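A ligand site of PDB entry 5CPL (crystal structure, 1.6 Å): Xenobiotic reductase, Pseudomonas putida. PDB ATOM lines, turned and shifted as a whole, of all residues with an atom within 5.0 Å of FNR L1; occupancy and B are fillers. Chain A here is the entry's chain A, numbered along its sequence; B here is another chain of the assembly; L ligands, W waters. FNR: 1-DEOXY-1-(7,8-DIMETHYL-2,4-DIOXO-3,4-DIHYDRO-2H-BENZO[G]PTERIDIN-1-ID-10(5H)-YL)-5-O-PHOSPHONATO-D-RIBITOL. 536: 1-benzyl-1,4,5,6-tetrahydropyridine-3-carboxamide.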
ATOM      1  N   PRO A  22       1.222  23.141  28.723  1.00  0.00           N
ATOM      2  CA  PRO A  22       1.082  22.576  27.391  1.00  0.00           C
ATOM      3  C   PRO A  22       0.075  23.305  26.566  1.00  0.00           C
ATOM      4  O   PRO A  22      -0.745  24.059  27.103  1.00  0.00           O
ATOM      5  CB  PRO A  22       0.611  21.160  27.659  1.00  0.00           C
ATOM      6  CG  PRO A  22      -0.266  21.299  28.879  1.00  0.00           C
ATOM      7  CD  PRO A  22       0.440  22.372  29.708  1.00  0.00           C
ATOM      8  N   PRO A  23       0.124  23.101  25.245  1.00  0.00           N
ATOM      9  CA  PRO A  23      -0.825  23.804  24.399  1.00  0.00           C
ATOM     10  C   PRO A  23      -2.261  23.458  24.783  1.00  0.00           C
ATOM     11  O   PRO A  23      -2.575  22.286  25.013  1.00  0.00           O
ATOM     12  CB  PRO A  23      -0.472  23.294  22.985  1.00  0.00           C
ATOM     13  CG  PRO A  23       0.204  21.933  23.217  1.00  0.00           C
ATOM     14  CD  PRO A  23       0.996  22.183  24.493  1.00  0.00           C
ATOM     15  N   MET A  24      -3.111  24.481  24.906  1.00  0.00           N
ATOM     16  CA  MET A  24      -4.525  24.261  25.191  1.00  0.00           C
ATOM     17  C   MET A  24      -5.379  25.206  24.356  1.00  0.00           C
ATOM     18  O   MET A  24      -5.477  26.407  24.628  1.00  0.00           O
ATOM     19  CB  MET A  24      -4.824  24.480  26.674  1.00  0.00           C
ATOM     20  CG  MET A  24      -4.326  23.338  27.563  1.00  0.00           C
ATOM     21  SD  MET A  24      -4.657  23.606  29.318  1.00  0.00           S
ATOM     22  CE  MET A  24      -3.556  24.967  29.692  1.00  0.00           C
ATOM     23  N   CYS A  25      -5.999  24.637  23.316  1.00  0.00           N
ATOM     24  CA  CYS A  25      -6.970  25.371  22.485  1.00  0.00           C
ATOM     25  C   CYS A  25      -7.986  26.123  23.327  1.00  0.00           C
ATOM     26  O   CYS A  25      -8.560  25.564  24.274  1.00  0.00           O
ATOM     27  CB  CYS A  25      -7.716  24.397  21.581  1.00  0.00           C
ATOM     28  SG  CYS A  25      -6.714  23.792  20.189  1.00  0.00           S
ATOM     29  N   GLN A  26      -8.225  27.374  22.956  1.00  0.00           N
ATOM     30  CA  GLN A  26      -9.183  28.250  23.630  1.00  0.00           C
ATOM     31  C   GLN A  26     -10.485  28.416  22.838  1.00  0.00           C
ATOM     32  O   GLN A  26     -11.490  28.852  23.392  1.00  0.00           O
ATOM     33  CB  GLN A  26      -8.528  29.602  23.869  1.00  0.00           C
ATOM     34  CG  GLN A  26      -7.353  29.510  24.794  1.00  0.00           C
ATOM     35  CD  GLN A  26      -7.769  29.026  26.158  1.00  0.00           C
ATOM     36  OE1 GLN A  26      -8.453  29.748  26.901  1.00  0.00           O
ATOM     37  NE2 GLN A  26      -7.384  27.809  26.478  1.00  0.00           N
ATOM     38  N   TYR A  27     -10.430  28.104  21.551  1.00  0.00           N
ATOM     39  CA  TYR A  27     -11.576  28.194  20.640  1.00  0.00           C
ATOM     40  C   TYR A  27     -12.204  29.590  20.632  1.00  0.00           C
ATOM     41  O   TYR A  27     -13.408  29.730  20.432  1.00  0.00           O
ATOM     42  CB  TYR A  27     -12.629  27.146  20.995  1.00  0.00           C
ATOM     43  CG  TYR A  27     -12.071  25.751  21.181  1.00  0.00           C
ATOM     44  CD1 TYR A  27     -11.933  24.885  20.100  1.00  0.00           C
ATOM     45  CD2 TYR A  27     -11.639  25.307  22.423  1.00  0.00           C
ATOM     46  CE1 TYR A  27     -11.391  23.624  20.250  1.00  0.00           C
ATOM     47  CE2 TYR A  27     -11.114  24.032  22.571  1.00  0.00           C
ATOM     48  CZ  TYR A  27     -11.005  23.201  21.494  1.00  0.00           C
ATOM     49  OH  TYR A  27     -10.478  21.948  21.621  1.00  0.00           O
ATOM     50  N   GLU A  56      -1.396  27.271  22.330  1.00  0.00           N
ATOM     51  CA  GLU A  56      -2.297  26.276  21.759  1.00  0.00           C
ATOM     52  C   GLU A  56      -2.035  25.916  20.302  1.00  0.00           C
ATOM     53  O   GLU A  56      -1.471  26.723  19.560  1.00  0.00           O
ATOM     54  CB  GLU A  56      -3.731  26.840  21.849  1.00  0.00           C
ATOM     55  CG  GLU A  56      -3.939  28.114  21.035  1.00  0.00           C
ATOM     56  CD  GLU A  56      -5.195  28.870  21.433  1.00  0.00           C
ATOM     57  OE1 GLU A  56      -6.286  28.554  20.915  1.00  0.00           O
ATOM     58  OE2 GLU A  56      -5.087  29.767  22.299  1.00  0.00           O
ATOM     59  N   ALA A  57      -2.508  24.736  19.898  1.00  0.00           N
ATOM     60  CA  ALA A  57      -2.504  24.316  18.499  1.00  0.00           C
ATOM     61  C   ALA A  57      -2.927  25.453  17.584  1.00  0.00           C
ATOM     62  O   ALA A  57      -4.079  25.882  17.621  1.00  0.00           O
ATOM     63  CB  ALA A  57      -3.423  23.114  18.315  1.00  0.00           C
ATOM     64  N   GLN A  99       2.764  25.606  19.490  1.00  0.00           N
ATOM     65  CA  GLN A  99       2.494  24.371  18.795  1.00  0.00           C
ATOM     66  C   GLN A  99       1.846  24.707  17.454  1.00  0.00           C
ATOM     67  O   GLN A  99       0.753  25.295  17.430  1.00  0.00           O
ATOM     68  CB  GLN A  99       1.571  23.486  19.638  1.00  0.00           C
ATOM     69  CG  GLN A  99       1.324  22.120  18.984  1.00  0.00           C
ATOM     70  CD  GLN A  99       0.214  21.353  19.672  1.00  0.00           C
ATOM     71  OE1 GLN A  99      -0.941  21.797  19.725  1.00  0.00           O
ATOM     72  NE2 GLN A  99       0.552  20.210  20.204  1.00  0.00           N
ATOM     73  N   GLU A 176       6.767  23.569  18.761  1.00  0.00           N
ATOM     74  CA  GLU A 176       6.291  22.188  18.894  1.00  0.00           C
ATOM     75  C   GLU A 176       5.467  21.817  17.665  1.00  0.00           C
ATOM     76  O   GLU A 176       4.451  22.436  17.381  1.00  0.00           O
ATOM     77  CB  GLU A 176       5.462  22.010  20.170  1.00  0.00           C
ATOM     78  CG  GLU A 176       5.075  20.567  20.461  1.00  0.00           C
ATOM     79  CD  GLU A 176       4.186  20.445  21.688  1.00  0.00           C
ATOM     80  OE1 GLU A 176       4.691  20.623  22.808  1.00  0.00           O
ATOM     81  OE2 GLU A 176       2.989  20.165  21.523  1.00  0.00           O
ATOM     82  N   HIS A 178       2.815  19.549  15.952  1.00  0.00           N
ATOM     83  CA  HIS A 178       1.732  18.735  16.468  1.00  0.00           C
ATOM     84  C   HIS A 178       1.524  17.470  15.635  1.00  0.00           C
ATOM     85  O   HIS A 178       0.738  17.456  14.681  1.00  0.00           O
ATOM     86  CB  HIS A 178       0.427  19.523  16.497  1.00  0.00           C
ATOM     87  CG  HIS A 178      -0.591  18.914  17.408  1.00  0.00           C
ATOM     88  ND1 HIS A 178      -0.450  17.643  17.935  1.00  0.00           N
ATOM     89  CD2 HIS A 178      -1.749  19.407  17.907  1.00  0.00           C
ATOM     90  CE1 HIS A 178      -1.479  17.390  18.734  1.00  0.00           C
ATOM     91  NE2 HIS A 178      -2.285  18.445  18.723  1.00  0.00           N
ATOM     92  N   HIS A 181      -2.520  13.158  18.639  1.00  0.00           N
ATOM     93  CA  HIS A 181      -3.958  13.336  18.895  1.00  0.00           C
ATOM     94  C   HIS A 181      -4.822  13.147  17.660  1.00  0.00           C
ATOM     95  O   HIS A 181      -5.955  13.655  17.595  1.00  0.00           O
ATOM     96  CB  HIS A 181      -4.203  14.698  19.542  1.00  0.00           C
ATOM     97  CG  HIS A 181      -3.484  14.856  20.845  1.00  0.00           C
ATOM     98  ND1 HIS A 181      -3.345  16.073  21.482  1.00  0.00           N
ATOM     99  CD2 HIS A 181      -2.823  13.958  21.596  1.00  0.00           C
ATOM    100  CE1 HIS A 181      -2.636  15.909  22.590  1.00  0.00           C
ATOM    101  NE2 HIS A 181      -2.319  14.625  22.681  1.00  0.00           N
ATOM    102  N   ARG A 231       5.110  16.963  19.421  1.00  0.00           N
ATOM    103  CA  ARG A 231       4.222  16.133  20.222  1.00  0.00           C
ATOM    104  C   ARG A 231       3.802  14.937  19.368  1.00  0.00           C
ATOM    105  O   ARG A 231       3.490  15.100  18.197  1.00  0.00           O
ATOM    106  CB  ARG A 231       3.004  16.929  20.722  1.00  0.00           C
ATOM    107  CG  ARG A 231       2.267  16.222  21.846  1.00  0.00           C
ATOM    108  CD  ARG A 231       1.272  17.144  22.576  1.00  0.00           C
ATOM    109  NE  ARG A 231       1.158  16.749  23.986  1.00  0.00           N
ATOM    110  CZ  ARG A 231       0.337  17.333  24.849  1.00  0.00           C
ATOM    111  NH1 ARG A 231      -0.526  18.256  24.459  1.00  0.00           N
ATOM    112  NH2 ARG A 231       0.359  16.958  26.121  1.00  0.00           N
ATOM    113  N   ALA A 301       1.926  14.762  30.026  1.00  0.00           N
ATOM    114  CA  ALA A 301       0.815  15.385  30.716  1.00  0.00           C
ATOM    115  C   ALA A 301      -0.215  14.333  31.098  1.00  0.00           C
ATOM    116  O   ALA A 301      -0.017  13.138  30.883  1.00  0.00           O
ATOM    117  CB  ALA A 301       0.181  16.459  29.818  1.00  0.00           C
ATOM    118  N   TRP A 302      -1.331  14.881  31.542  1.00  0.00           N
ATOM    119  CA  TRP A 302      -2.506  14.159  31.971  1.00  0.00           C
ATOM    120  C   TRP A 302      -2.602  13.655  33.571  1.00  0.00           C
ATOM    121  O   TRP A 302      -2.022  12.631  34.075  1.00  0.00           O
ATOM    122  CB  TRP A 302      -2.707  12.995  30.928  1.00  0.00           C
ATOM    123  CG  TRP A 302      -2.568  13.348  29.323  1.00  0.00           C
ATOM    124  CD1 TRP A 302      -1.449  13.153  28.494  1.00  0.00           C
ATOM    125  CD2 TRP A 302      -3.591  13.865  28.426  1.00  0.00           C
ATOM    126  NE1 TRP A 302      -1.731  13.534  27.204  1.00  0.00           N
ATOM    127  CE2 TRP A 302      -3.036  13.976  27.127  1.00  0.00           C
ATOM    128  CE3 TRP A 302      -4.933  14.253  28.603  1.00  0.00           C
ATOM    129  CZ2 TRP A 302      -3.760  14.453  26.020  1.00  0.00           C
ATOM    130  CZ3 TRP A 302      -5.644  14.728  27.495  1.00  0.00           C
ATOM    131  CH2 TRP A 302      -5.052  14.826  26.229  1.00  0.00           C
ATOM    132  N   GLY A 303      -2.879  14.695  34.431  1.00  0.00           N
ATOM    133  CA  GLY A 303      -2.939  14.428  35.861  1.00  0.00           C
ATOM    134  C   GLY A 303      -1.913  15.051  36.822  1.00  0.00           C
ATOM    135  O   GLY A 303      -2.027  14.901  38.052  1.00  0.00           O
ATOM    136  N   PHE A 304      -0.912  15.741  36.288  1.00  0.00           N
ATOM    137  CA  PHE A 304       0.183  16.246  37.124  1.00  0.00           C
ATOM    138  C   PHE A 304      -0.118  17.530  37.871  1.00  0.00           C
ATOM    139  O   PHE A 304       0.785  18.120  38.476  1.00  0.00           O
ATOM    140  CB  PHE A 304       1.439  16.432  36.250  1.00  0.00           C
ATOM    141  CG  PHE A 304       2.005  15.145  35.737  1.00  0.00           C
ATOM    142  CD1 PHE A 304       2.712  14.298  36.586  1.00  0.00           C
ATOM    143  CD2 PHE A 304       1.794  14.732  34.438  1.00  0.00           C
ATOM    144  CE1 PHE A 304       3.228  13.098  36.142  1.00  0.00           C
ATOM    145  CE2 PHE A 304       2.312  13.546  33.979  1.00  0.00           C
ATOM    146  CZ  PHE A 304       3.028  12.691  34.864  1.00  0.00           C
ATOM    147  N   SER A 323       4.250  18.806  32.154  1.00  0.00           N
ATOM    148  CA  SER A 323       3.221  19.667  31.557  1.00  0.00           C
ATOM    149  C   SER A 323       1.977  19.589  32.413  1.00  0.00           C
ATOM    150  O   SER A 323       1.493  18.510  32.747  1.00  0.00           O
ATOM    151  CB  SER A 323       2.933  19.253  30.108  1.00  0.00           C
ATOM    152  OG  SER A 323       4.098  19.453  29.325  1.00  0.00           O
ATOM    153  N   VAL A 324       1.488  20.763  32.805  1.00  0.00           N
ATOM    154  CA  VAL A 324       0.323  20.909  33.694  1.00  0.00           C
ATOM    155  C   VAL A 324      -0.697  21.817  33.018  1.00  0.00           C
ATOM    156  O   VAL A 324      -0.500  23.036  32.924  1.00  0.00           O
ATOM    157  CB  VAL A 324       0.733  21.481  35.057  1.00  0.00           C
ATOM    158  CG1 VAL A 324      -0.483  21.656  35.970  1.00  0.00           C
ATOM    159  CG2 VAL A 324       1.765  20.568  35.714  1.00  0.00           C
ATOM    160  N   GLY A 325      -1.793  21.221  32.531  1.00  0.00           N
ATOM    161  CA  GLY A 325      -2.751  21.946  31.707  1.00  0.00           C
ATOM    162  C   GLY A 325      -3.971  22.457  32.445  1.00  0.00           C
ATOM    163  O   GLY A 325      -4.078  23.655  32.783  1.00  0.00           O
ATOM    164  N   ARG A 326      -4.926  21.570  32.686  1.00  0.00           N
ATOM    165  CA  ARG A 326      -6.191  21.993  33.261  1.00  0.00           C
ATOM    166  C   ARG A 326      -6.053  22.697  34.618  1.00  0.00           C
ATOM    167  O   ARG A 326      -6.808  23.607  34.905  1.00  0.00           O
ATOM    168  CB  ARG A 326      -7.144  20.818  33.371  1.00  0.00           C
ATOM    169  CG  ARG A 326      -7.815  20.507  32.032  1.00  0.00           C
ATOM    170  CD  ARG A 326      -8.491  19.145  31.980  1.00  0.00           C
ATOM    171  NE  ARG A 326      -7.519  18.088  32.090  1.00  0.00           N
ATOM    172  CZ  ARG A 326      -7.821  16.793  32.054  1.00  0.00           C
ATOM    173  NH1 ARG A 326      -9.098  16.424  31.906  1.00  0.00           N
ATOM    174  NH2 ARG A 326      -6.866  15.874  32.174  1.00  0.00           N
ATOM    175  N   ALA A 327      -5.076  22.314  35.446  1.00  0.00           N
ATOM    176  CA  ALA A 327      -4.862  23.000  36.721  1.00  0.00           C
ATOM    177  C   ALA A 327      -4.553  24.484  36.520  1.00  0.00           C
ATOM    178  O   ALA A 327      -4.859  25.280  37.403  1.00  0.00           O
ATOM    179  CB  ALA A 327      -3.765  22.345  37.501  1.00  0.00           C
ATOM    180  N   LEU A 329      -5.891  26.250  33.979  1.00  0.00           N
ATOM    181  CA  LEU A 329      -7.169  26.854  33.628  1.00  0.00           C
ATOM    182  C   LEU A 329      -7.930  27.167  34.920  1.00  0.00           C
ATOM    183  O   LEU A 329      -8.581  28.211  35.039  1.00  0.00           O
ATOM    184  CB  LEU A 329      -7.999  25.932  32.725  1.00  0.00           C
ATOM    185  CG  LEU A 329      -7.337  25.430  31.433  1.00  0.00           C
ATOM    186  CD1 LEU A 329      -8.343  24.592  30.656  1.00  0.00           C
ATOM    187  CD2 LEU A 329      -6.793  26.541  30.569  1.00  0.00           C
ATOM    188  N   PRO B 354     -14.238  28.614  27.833  1.00  0.00           N
ATOM    189  CA  PRO B 354     -13.006  27.912  27.458  1.00  0.00           C
ATOM    190  C   PRO B 354     -12.314  27.262  28.631  1.00  0.00           C
ATOM    191  O   PRO B 354     -11.455  26.396  28.454  1.00  0.00           O
ATOM    192  CB  PRO B 354     -12.131  29.016  26.845  1.00  0.00           C
ATOM    193  CG  PRO B 354     -13.095  30.080  26.416  1.00  0.00           C
ATOM    194  CD  PRO B 354     -14.231  30.026  27.390  1.00  0.00           C
ATOM    195  N   TRP B 358     -14.045  22.354  30.461  1.00  0.00           N
ATOM    196  CA  TRP B 358     -13.066  21.326  30.742  1.00  0.00           C
ATOM    197  C   TRP B 358     -12.953  21.007  32.207  1.00  0.00           C
ATOM    198  O   TRP B 358     -12.416  19.966  32.576  1.00  0.00           O
ATOM    199  CB  TRP B 358     -11.709  21.748  30.214  1.00  0.00           C
ATOM    200  CG  TRP B 358     -11.748  22.004  28.750  1.00  0.00           C
ATOM    201  CD1 TRP B 358     -11.915  23.222  28.111  1.00  0.00           C
ATOM    202  CD2 TRP B 358     -11.662  21.018  27.728  1.00  0.00           C
ATOM    203  NE1 TRP B 358     -11.917  23.026  26.765  1.00  0.00           N
ATOM    204  CE2 TRP B 358     -11.749  21.691  26.494  1.00  0.00           C
ATOM    205  CE3 TRP B 358     -11.480  19.635  27.721  1.00  0.00           C
ATOM    206  CZ2 TRP B 358     -11.673  21.030  25.270  1.00  0.00           C
ATOM    207  CZ3 TRP B 358     -11.418  18.976  26.499  1.00  0.00           C
ATOM    208  CH2 TRP B 358     -11.506  19.667  25.297  1.00  0.00           C
HETATM  209  C9A FNR L   1      -5.933  20.333  25.379  1.00  0.00           C
HETATM  210  N10 FNR L   1      -4.775  19.573  24.940  1.00  0.00           N
HETATM  211  CAA FNR L   1      -4.093  19.951  23.709  1.00  0.00           C
HETATM  212  N1  FNR L   1      -3.106  19.202  23.264  1.00  0.00           N
HETATM  213  C2  FNR L   1      -2.356  19.615  22.243  1.00  0.00           C
HETATM  214  O2  FNR L   1      -1.454  18.925  21.863  1.00  0.00           O
HETATM  215  N3  FNR L   1      -2.658  20.819  21.662  1.00  0.00           N
HETATM  216  C4  FNR L   1      -3.687  21.561  22.054  1.00  0.00           C
HETATM  217  O4  FNR L   1      -3.914  22.652  21.565  1.00  0.00           O
HETATM  218  C4A FNR L   1      -4.551  20.971  22.957  1.00  0.00           C
HETATM  219  N5  FNR L   1      -5.759  21.665  23.383  1.00  0.00           N
HETATM  220  C5A FNR L   1      -6.427  21.361  24.619  1.00  0.00           C
HETATM  221  C6  FNR L   1      -7.302  22.290  25.141  1.00  0.00           C
HETATM  222  C7  FNR L   1      -7.788  22.097  26.420  1.00  0.00           C
HETATM  223  C7M FNR L   1      -8.716  23.166  26.950  1.00  0.00           C
HETATM  224  C8  FNR L   1      -7.384  20.992  27.138  1.00  0.00           C
HETATM  225  C8M FNR L   1      -7.908  20.768  28.539  1.00  0.00           C
HETATM  226  C9  FNR L   1      -6.518  20.090  26.613  1.00  0.00           C
HETATM  227  C1' FNR L   1      -4.223  18.539  25.800  1.00  0.00           C
HETATM  228  C2' FNR L   1      -3.351  19.208  26.878  1.00  0.00           C
HETATM  229  O2' FNR L   1      -2.199  19.766  26.282  1.00  0.00           O
HETATM  230  C3' FNR L   1      -2.913  18.234  27.972  1.00  0.00           C
HETATM  231  O3' FNR L   1      -2.181  17.158  27.430  1.00  0.00           O
HETATM  232  C4' FNR L   1      -4.110  17.694  28.752  1.00  0.00           C
HETATM  233  O4' FNR L   1      -4.915  18.764  29.209  1.00  0.00           O
HETATM  234  C5' FNR L   1      -3.678  16.810  29.921  1.00  0.00           C
HETATM  235  O5' FNR L   1      -2.946  17.512  30.892  1.00  0.00           O
HETATM  236  P   FNR L   1      -3.719  17.965  32.252  1.00  0.00           P
HETATM  237  O1P FNR L   1      -4.865  18.879  31.855  1.00  0.00           O
HETATM  238  O2P FNR L   1      -2.669  18.684  33.042  1.00  0.00           O
HETATM  239  O3P FNR L   1      -4.252  16.737  32.986  1.00  0.00           O
HETATM  240  C1  536 L   2      -7.489  15.889  23.547  1.00  0.00           C
HETATM  241  N2  536 L   2      -7.650  17.159  22.876  1.00  0.00           N
HETATM  242  C3  536 L   2      -6.516  17.732  22.280  1.00  0.00           C
HETATM  243  C4  536 L   2      -6.665  18.805  21.496  1.00  0.00           C
HETATM  244  C5  536 L   2      -7.857  19.747  21.505  1.00  0.00           C
HETATM  245  C6  536 L   2      -8.817  19.326  22.611  1.00  0.00           C
HETATM  246  C7  536 L   2      -8.914  17.814  22.732  1.00  0.00           C
HETATM  247  C8  536 L   2      -5.507  19.147  20.586  1.00  0.00           C
HETATM  248  O9  536 L   2      -4.502  18.446  20.502  1.00  0.00           O
HETATM  249  N10 536 L   2      -5.633  20.402  19.930  1.00  0.00           N
HETATM  250  C11 536 L   2      -8.061  15.901  24.982  1.00  0.00           C
HETATM  251  C12 536 L   2      -8.737  14.815  25.434  1.00  0.00           C
HETATM  252  C13 536 L   2      -9.313  14.815  26.841  1.00  0.00           C
HETATM  253  C14 536 L   2      -9.148  15.895  27.654  1.00  0.00           C
HETATM  254  C15 536 L   2      -8.384  17.092  27.152  1.00  0.00           C
HETATM  255  C16 536 L   2      -7.879  17.104  25.892  1.00  0.00           C
HETATM  256  O   HOH W   1      -5.818  17.009  35.212  1.00  0.00           O
HETATM  257  O   HOH W   2      -0.664  17.025  33.667  1.00  0.00           O
HETATM  258  O   HOH W   3      -3.565  19.891  35.388  1.00  0.00           O
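SG of Cys 25 is in hydrogen-bond range of O4 of FNR L1 (3.3 Å). The guanidinium group of Arg 231 sits at hydrogen-bond distance from an oxygen (O2) of FNR L1 (2.8 Å). ND1 of His 181 sits close to O2 of FNR L1 (3.4 Å). N of Gly 303 is in hydrogen-bond range of O3P of FNR L1 (2.9 Å). A ring nitrogen (NE2) of His 178 is in hydrogen-bond range of an oxygen (O2) of FNR L1 (3.3 Å). NE of Arg 326 lies within salt-bridge range of O1P of FNR L1 (2.8 Å). An oxygen (O9) of 536 L2 sits at hydrogen-bond distance from a ring nitrogen (ND1) of His 181 (2.8 Å). The backbone NH (N) of Trp 302 lies within hydrogen-bond range of an oxygen (O5') of FNR L1, 3.2 Å away. The backbone NH (N) of Cys 25 lies close to an oxygen (O4) of FNR L1, at 3.4 Å. The side-chain amide oxygen (OE1) of Gln 99 lies within hydrogen-bond range of a nitrogen (N3) of FNR L1, 2.8 Å away. An oxygen (O9) of 536 L2 lies within hydrogen-bond range of a ring nitrogen (NE2) of His 178 (2.8 Å). N of Ala 57 is in hydrogen-bond range of O4 of FNR L1 (3.0 Å). The backbone NH (N) of Gly 325 lies within hydrogen-bond range of an oxygen (O2P) of FNR L1, 2.7 Å away. SG of Cys 25 lies within hydrogen-bond range of N10 of 536 L2. The backbone carbonyl oxygen (O) of Pro 23 lies within hydrogen-bond range of an oxygen (O2') of FNR L1 (2.8 Å). O1P of FNR L1 sits at hydrogen-bond distance from N of Arg 326 (2.8 Å).
N1 of FNR L1 lies close to O9 of 536 L2, at 3.2 Å.
NE2 of Gln 99 lies within hydrogen-bond range of OE2 of Glu 176 (2.8 Å). The side-chain amide nitrogen (NE2) of Gln 26 sits at hydrogen-bond distance from the backbone carbonyl oxygen (O) of Met 24. OE1 of Glu 56 is in hydrogen-bond range of N of Gln 26 (3.1 Å). OE1 of Gln 99 lies close to N of Ala 57, 3.3 Å away.
Pro 22 touches FNR L1 (CB to O2', 3.4 Å). CA of Met 24 touches N5 of FNR L1, at 3.4 Å. C of Glu 56 touches O4 of FNR L1, 3.97 Å away. Ala 301 touches FNR L1. Val 324 touches FNR L1 (C to O2P, 3.7 Å). CD1 of Leu 329 touches C7M of FNR L1, 3.99 Å away. NE1 of Trp 358 of chain B touches C7M of FNR L1, at 3.2 Å. Within 4 Å of FNR L1: Pro 22, Pro 23, Met 24, Cys 25, Glu 56, Ala 57, Gln 99, His 178, His 181, Arg 231, Ala 301, Trp 302, Gly 303, Val 324, Gly 325, Arg 326, Leu 329 and Trp 358 of chain B.
Water W1 lies within hydrogen-bond range of O3P of FNR L1 (2.7 Å) and NH2 of Arg 326 (3.4 Å). Water W3 lies within hydrogen-bond range of O2P of FNR L1, N of Ala 327 and N of Arg 326.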
